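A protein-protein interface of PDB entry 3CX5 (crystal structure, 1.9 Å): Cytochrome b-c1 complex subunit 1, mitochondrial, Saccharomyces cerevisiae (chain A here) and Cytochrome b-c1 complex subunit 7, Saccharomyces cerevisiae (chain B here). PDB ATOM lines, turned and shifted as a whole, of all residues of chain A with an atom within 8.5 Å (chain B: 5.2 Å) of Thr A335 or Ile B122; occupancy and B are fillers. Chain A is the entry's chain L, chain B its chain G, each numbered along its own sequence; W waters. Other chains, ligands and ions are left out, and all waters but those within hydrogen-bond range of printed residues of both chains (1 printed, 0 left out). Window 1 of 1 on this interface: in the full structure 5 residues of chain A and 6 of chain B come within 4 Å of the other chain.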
ATOM      1  N   ILE A 258      -6.980 -15.718  17.920  1.00  0.00           N
ATOM      2  CA  ILE A 258      -5.979 -14.781  17.421  1.00  0.00           C
ATOM      3  C   ILE A 258      -6.415 -14.233  16.053  1.00  0.00           C
ATOM      4  O   ILE A 258      -6.328 -13.031  15.804  1.00  0.00           O
ATOM      5  CB  ILE A 258      -4.587 -15.448  17.315  1.00  0.00           C
ATOM      6  CG1 ILE A 258      -4.026 -15.699  18.717  1.00  0.00           C
ATOM      7  CG2 ILE A 258      -3.622 -14.579  16.505  1.00  0.00           C
ATOM      8  CD1 ILE A 258      -2.716 -16.439  18.721  1.00  0.00           C
ATOM      9  N   GLY A 273      -7.886  -5.904  16.176  1.00  0.00           N
ATOM     10  CA  GLY A 273      -6.447  -6.093  16.235  1.00  0.00           C
ATOM     11  C   GLY A 273      -6.033  -7.431  15.644  1.00  0.00           C
ATOM     12  O   GLY A 273      -5.466  -8.290  16.336  1.00  0.00           O
ATOM     13  N   LYS A 275      -3.937  -8.853  12.378  1.00  0.00           N
ATOM     14  CA  LYS A 275      -3.028  -8.505  11.289  1.00  0.00           C
ATOM     15  C   LYS A 275      -3.519  -8.932   9.908  1.00  0.00           C
ATOM     16  O   LYS A 275      -3.286  -8.229   8.925  1.00  0.00           O
ATOM     17  CB  LYS A 275      -1.620  -9.030  11.566  1.00  0.00           C
ATOM     18  CG  LYS A 275      -1.000  -8.412  12.824  1.00  0.00           C
ATOM     19  CD  LYS A 275       0.442  -8.853  13.043  1.00  0.00           C
ATOM     20  CE  LYS A 275       0.969  -8.378  14.401  1.00  0.00           C
ATOM     21  NZ  LYS A 275       0.856  -6.895  14.593  1.00  0.00           N
ATOM     22  N   SER A 331       6.430 -16.716  14.520  1.00  0.00           N
ATOM     23  CA  SER A 331       6.520 -15.322  14.946  1.00  0.00           C
ATOM     24  C   SER A 331       5.356 -14.667  15.676  1.00  0.00           C
ATOM     25  O   SER A 331       5.333 -13.443  15.801  1.00  0.00           O
ATOM     26  CB  SER A 331       6.856 -14.475  13.719  1.00  0.00           C
ATOM     27  OG  SER A 331       5.842 -14.634  12.742  1.00  0.00           O
ATOM     28  N   VAL A 332       4.390 -15.451  16.142  1.00  0.00           N
ATOM     29  CA  VAL A 332       3.250 -14.891  16.862  1.00  0.00           C
ATOM     30  C   VAL A 332       3.772 -14.050  18.033  1.00  0.00           C
ATOM     31  O   VAL A 332       4.675 -14.473  18.762  1.00  0.00           O
ATOM     32  CB  VAL A 332       2.292 -16.007  17.351  1.00  0.00           C
ATOM     33  CG1 VAL A 332       3.022 -16.991  18.257  1.00  0.00           C
ATOM     34  CG2 VAL A 332       1.076 -15.403  18.036  1.00  0.00           C
ATOM     35  N   THR A 333       3.258 -12.830  18.159  1.00  0.00           N
ATOM     36  CA  THR A 333       3.703 -11.918  19.205  1.00  0.00           C
ATOM     37  C   THR A 333       2.986 -12.066  20.540  1.00  0.00           C
ATOM     38  O   THR A 333       1.869 -12.586  20.624  1.00  0.00           O
ATOM     39  CB  THR A 333       3.587 -10.434  18.766  1.00  0.00           C
ATOM     40  OG1 THR A 333       2.206 -10.050  18.716  1.00  0.00           O
ATOM     41  CG2 THR A 333       4.227 -10.218  17.399  1.00  0.00           C
ATOM     42  N   ASP A 334       3.634 -11.538  21.573  1.00  0.00           N
ATOM     43  CA  ASP A 334       3.128 -11.552  22.937  1.00  0.00           C
ATOM     44  C   ASP A 334       1.782 -10.832  23.021  1.00  0.00           C
ATOM     45  O   ASP A 334       0.849 -11.314  23.660  1.00  0.00           O
ATOM     46  CB  ASP A 334       4.157 -10.877  23.847  1.00  0.00           C
ATOM     47  CG  ASP A 334       3.842 -11.050  25.312  1.00  0.00           C
ATOM     48  OD1 ASP A 334       4.217 -12.101  25.880  1.00  0.00           O
ATOM     49  OD2 ASP A 334       3.230 -10.128  25.895  1.00  0.00           O
ATOM     50  N   THR A 335       1.674  -9.693  22.345  1.00  0.00           N
ATOM     51  CA  THR A 335       0.437  -8.924  22.340  1.00  0.00           C
ATOM     52  C   THR A 335      -0.716  -9.679  21.688  1.00  0.00           C
ATOM     53  O   THR A 335      -1.864  -9.574  22.137  1.00  0.00           O
ATOM     54  CB  THR A 335       0.636  -7.566  21.655  1.00  0.00           C
ATOM     55  OG1 THR A 335       1.485  -6.755  22.476  1.00  0.00           O
ATOM     56  CG2 THR A 335      -0.699  -6.857  21.437  1.00  0.00           C
ATOM     57  N   GLU A 336      -0.417 -10.428  20.625  1.00  0.00           N
ATOM     58  CA  GLU A 336      -1.447 -11.210  19.943  1.00  0.00           C
ATOM     59  C   GLU A 336      -1.981 -12.288  20.891  1.00  0.00           C
ATOM     60  O   GLU A 336      -3.182 -12.537  20.945  1.00  0.00           O
ATOM     61  CB  GLU A 336      -0.897 -11.849  18.654  1.00  0.00           C
ATOM     62  CG  GLU A 336      -0.709 -10.862  17.494  1.00  0.00           C
ATOM     63  CD  GLU A 336      -0.015 -11.484  16.278  1.00  0.00           C
ATOM     64  OE1 GLU A 336       1.189 -11.801  16.360  1.00  0.00           O
ATOM     65  OE2 GLU A 336      -0.675 -11.644  15.230  1.00  0.00           O
ATOM     66  N   VAL A 337      -1.084 -12.909  21.653  1.00  0.00           N
ATOM     67  CA  VAL A 337      -1.485 -13.945  22.600  1.00  0.00           C
ATOM     68  C   VAL A 337      -2.292 -13.351  23.751  1.00  0.00           C
ATOM     69  O   VAL A 337      -3.290 -13.932  24.174  1.00  0.00           O
ATOM     70  CB  VAL A 337      -0.268 -14.730  23.141  1.00  0.00           C
ATOM     71  CG1 VAL A 337      -0.682 -15.624  24.307  1.00  0.00           C
ATOM     72  CG2 VAL A 337       0.322 -15.590  22.031  1.00  0.00           C
ATOM     73  N   GLU A 338      -1.894 -12.170  24.219  1.00  0.00           N
ATOM     74  CA  GLU A 338      -2.610 -11.514  25.310  1.00  0.00           C
ATOM     75  C   GLU A 338      -4.006 -11.078  24.891  1.00  0.00           C
ATOM     76  O   GLU A 338      -4.970 -11.275  25.636  1.00  0.00           O
ATOM     77  CB  GLU A 338      -1.810 -10.330  25.860  1.00  0.00           C
ATOM     78  CG  GLU A 338      -0.551 -10.754  26.628  1.00  0.00           C
ATOM     79  CD  GLU A 338      -0.867 -11.687  27.791  1.00  0.00           C
ATOM     80  OE1 GLU A 338      -0.260 -12.780  27.863  1.00  0.00           O
ATOM     81  OE2 GLU A 338      -1.735 -11.330  28.620  1.00  0.00           O
ATOM     82  N   ARG A 339      -4.122 -10.532  23.683  1.00  0.00           N
ATOM     83  CA  ARG A 339      -5.414 -10.091  23.173  1.00  0.00           C
ATOM     84  C   ARG A 339      -6.343 -11.297  23.065  1.00  0.00           C
ATOM     85  O   ARG A 339      -7.510 -11.226  23.452  1.00  0.00           O
ATOM     86  CB  ARG A 339      -5.275  -9.436  21.794  1.00  0.00           C
ATOM     87  CG  ARG A 339      -6.538  -8.695  21.347  1.00  0.00           C
ATOM     88  CD  ARG A 339      -6.594  -8.465  19.840  1.00  0.00           C
ATOM     89  NE  ARG A 339      -6.729  -9.742  19.166  1.00  0.00           N
ATOM     90  CZ  ARG A 339      -7.767 -10.118  18.426  1.00  0.00           C
ATOM     91  NH1 ARG A 339      -7.759 -11.325  17.895  1.00  0.00           N
ATOM     92  NH2 ARG A 339      -8.778  -9.290  18.181  1.00  0.00           N
ATOM     93  N   ALA A 340      -5.803 -12.409  22.571  1.00  0.00           N
ATOM     94  CA  ALA A 340      -6.583 -13.632  22.404  1.00  0.00           C
ATOM     95  C   ALA A 340      -7.097 -14.184  23.733  1.00  0.00           C
ATOM     96  O   ALA A 340      -8.217 -14.680  23.793  1.00  0.00           O
ATOM     97  CB  ALA A 340      -5.775 -14.688  21.661  1.00  0.00           C
ATOM     98  N   LYS A 341      -6.278 -14.106  24.783  1.00  0.00           N
ATOM     99  CA  LYS A 341      -6.668 -14.580  26.117  1.00  0.00           C
ATOM    100  C   LYS A 341      -7.929 -13.867  26.577  1.00  0.00           C
ATOM    101  O   LYS A 341      -8.905 -14.502  26.974  1.00  0.00           O
ATOM    102  CB  LYS A 341      -5.555 -14.322  27.137  1.00  0.00           C
ATOM    103  CG  LYS A 341      -4.429 -15.318  27.098  1.00  0.00           C
ATOM    104  CD  LYS A 341      -3.322 -14.935  28.062  1.00  0.00           C
ATOM    105  CE  LYS A 341      -2.198 -15.948  28.005  1.00  0.00           C
ATOM    106  NZ  LYS A 341      -1.057 -15.560  28.873  1.00  0.00           N
ATOM    107  N   SER A 342      -7.902 -12.540  26.497  1.00  0.00           N
ATOM    108  CA  SER A 342      -9.028 -11.711  26.895  1.00  0.00           C
ATOM    109  C   SER A 342     -10.288 -12.024  26.108  1.00  0.00           C
ATOM    110  O   SER A 342     -11.372 -12.150  26.681  1.00  0.00           O
ATOM    111  CB  SER A 342      -8.682 -10.237  26.721  1.00  0.00           C
ATOM    112  OG  SER A 342      -7.610  -9.880  27.566  1.00  0.00           O
ATOM    113  N   VAL A 389       3.566 -17.818  24.683  1.00  0.00           N
ATOM    114  CA  VAL A 389       3.889 -17.722  23.267  1.00  0.00           C
ATOM    115  C   VAL A 389       4.521 -19.039  22.836  1.00  0.00           C
ATOM    116  O   VAL A 389       4.221 -19.554  21.757  1.00  0.00           O
ATOM    117  CB  VAL A 389       4.845 -16.537  22.986  1.00  0.00           C
ATOM    118  CG1 VAL A 389       5.435 -16.641  21.590  1.00  0.00           C
ATOM    119  CG2 VAL A 389       4.090 -15.221  23.126  1.00  0.00           C
ATOM    120  N   GLU B 118       0.978   2.725  16.096  1.00  0.00           N
ATOM    121  CA  GLU B 118       1.329   2.540  17.505  1.00  0.00           C
ATOM    122  C   GLU B 118       0.520   1.391  18.086  1.00  0.00           C
ATOM    123  O   GLU B 118       1.067   0.523  18.764  1.00  0.00           O
ATOM    124  CB  GLU B 118       1.084   3.826  18.301  1.00  0.00           C
ATOM    125  CG  GLU B 118       2.033   4.953  17.914  1.00  0.00           C
ATOM    126  CD  GLU B 118       1.660   6.306  18.504  1.00  0.00           C
ATOM    127  OE1 GLU B 118       0.466   6.547  18.805  1.00  0.00           O
ATOM    128  OE2 GLU B 118       2.577   7.147  18.643  1.00  0.00           O
ATOM    129  N   LEU B 119      -0.772   1.357  17.765  1.00  0.00           N
ATOM    130  CA  LEU B 119      -1.652   0.302  18.257  1.00  0.00           C
ATOM    131  C   LEU B 119      -1.327  -1.068  17.661  1.00  0.00           C
ATOM    132  O   LEU B 119      -1.482  -2.091  18.331  1.00  0.00           O
ATOM    133  CB  LEU B 119      -3.117   0.678  18.023  1.00  0.00           C
ATOM    134  CG  LEU B 119      -3.608   1.848  18.890  1.00  0.00           C
ATOM    135  CD1 LEU B 119      -4.953   2.346  18.397  1.00  0.00           C
ATOM    136  CD2 LEU B 119      -3.693   1.428  20.356  1.00  0.00           C
ATOM    137  N   ASP B 120      -0.854  -1.088  16.414  1.00  0.00           N
ATOM    138  CA  ASP B 120      -0.485  -2.342  15.753  1.00  0.00           C
ATOM    139  C   ASP B 120       0.777  -2.931  16.379  1.00  0.00           C
ATOM    140  O   ASP B 120       1.041  -4.124  16.246  1.00  0.00           O
ATOM    141  CB  ASP B 120      -0.239  -2.128  14.249  1.00  0.00           C
ATOM    142  CG  ASP B 120      -1.524  -1.957  13.451  1.00  0.00           C
ATOM    143  OD1 ASP B 120      -2.624  -2.121  14.018  1.00  0.00           O
ATOM    144  OD2 ASP B 120      -1.433  -1.665  12.237  1.00  0.00           O
ATOM    145  N   ASN B 121       1.552  -2.096  17.064  1.00  0.00           N
ATOM    146  CA  ASN B 121       2.793  -2.551  17.685  1.00  0.00           C
ATOM    147  C   ASN B 121       2.865  -2.365  19.202  1.00  0.00           C
ATOM    148  O   ASN B 121       3.958  -2.333  19.776  1.00  0.00           O
ATOM    149  CB  ASN B 121       3.989  -1.861  17.021  1.00  0.00           C
ATOM    150  CG  ASN B 121       4.078  -2.154  15.534  1.00  0.00           C
ATOM    151  OD1 ASN B 121       4.062  -3.313  15.117  1.00  0.00           O
ATOM    152  ND2 ASN B 121       4.152  -1.104  14.730  1.00  0.00           N
ATOM    153  N   ILE B 122       1.714  -2.253  19.857  1.00  0.00           N
ATOM    154  CA  ILE B 122       1.699  -2.080  21.308  1.00  0.00           C
ATOM    155  C   ILE B 122       2.263  -3.282  22.059  1.00  0.00           C
ATOM    156  O   ILE B 122       2.096  -4.428  21.645  1.00  0.00           O
ATOM    157  CB  ILE B 122       0.282  -1.815  21.858  1.00  0.00           C
ATOM    158  CG1 ILE B 122      -0.699  -2.857  21.321  1.00  0.00           C
ATOM    159  CG2 ILE B 122      -0.141  -0.384  21.574  1.00  0.00           C
ATOM    160  CD1 ILE B 122      -2.133  -2.609  21.717  1.00  0.00           C
ATOM    161  N   GLU B 123       2.984  -2.999  23.138  1.00  0.00           N
ATOM    162  CA  GLU B 123       3.546  -4.041  23.982  1.00  0.00           C
ATOM    163  C   GLU B 123       2.695  -4.065  25.244  1.00  0.00           C
ATOM    164  O   GLU B 123       2.184  -3.029  25.669  1.00  0.00           O
ATOM    165  CB  GLU B 123       4.998  -3.731  24.352  1.00  0.00           C
ATOM    166  CG  GLU B 123       5.993  -3.859  23.216  1.00  0.00           C
ATOM    167  CD  GLU B 123       7.435  -3.818  23.705  1.00  0.00           C
ATOM    168  OE1 GLU B 123       7.883  -2.742  24.163  1.00  0.00           O
ATOM    169  OE2 GLU B 123       8.121  -4.865  23.639  1.00  0.00           O
ATOM    170  N   VAL B 124       2.489  -5.250  25.806  1.00  0.00           N
ATOM    171  CA  VAL B 124       1.704  -5.368  27.026  1.00  0.00           C
ATOM    172  C   VAL B 124       2.622  -5.653  28.203  1.00  0.00           C
ATOM    173  O   VAL B 124       3.386  -6.618  28.189  1.00  0.00           O
ATOM    174  CB  VAL B 124       0.616  -6.461  26.929  1.00  0.00           C
ATOM    175  CG1 VAL B 124      -0.488  -6.024  25.977  1.00  0.00           C
ATOM    176  CG2 VAL B 124       1.223  -7.773  26.471  1.00  0.00           C
HETATM  177  O   HOH W   1       3.778  -7.445  24.564  1.00  0.00           O
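NZ of Lys A275 is in hydrogen-bond range of O of Asp B120, at 3.2 Å.
The side-chain hydroxyl (OG1) of Thr A335 is in hydrogen-bond range of the backbone carbonyl oxygen (O) of Ile B122 (2.5 Å).
Of the printed residues of chain A, Asp B120 touches Lys A275.
Of the printed residues of chain A, Glu B123 touches Thr A335.
Of the 16 printed residues of chain A, 4 touch a printed residue of chain B.
Among the printed residues, no Asp or Glu carboxylate lies within 4 Å of a Lys or Arg side-chain nitrogen of the other chain.
Water W1 lies within hydrogen-bond range of the backbone NH (N) of Val B124 (2.8 Å), the side-chain carboxylate (OD2) of Asp A334 (3.0 Å) and the side-chain hydroxyl (OG1) of Thr A335 (3.2 Å).
NZ of Lys A341 lies within salt-bridge range of OE1 of Glu A338, at 3.1 Å.
Among the printed residues, pairs that only touch across the chains: Asp A334 with Val B124 (3.1 Å), Glu A338 with Val B124 (3.5 Å), Thr A335 with Glu B123 (3.7 Å) and Thr A335 with Val B124 (3.8 Å).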
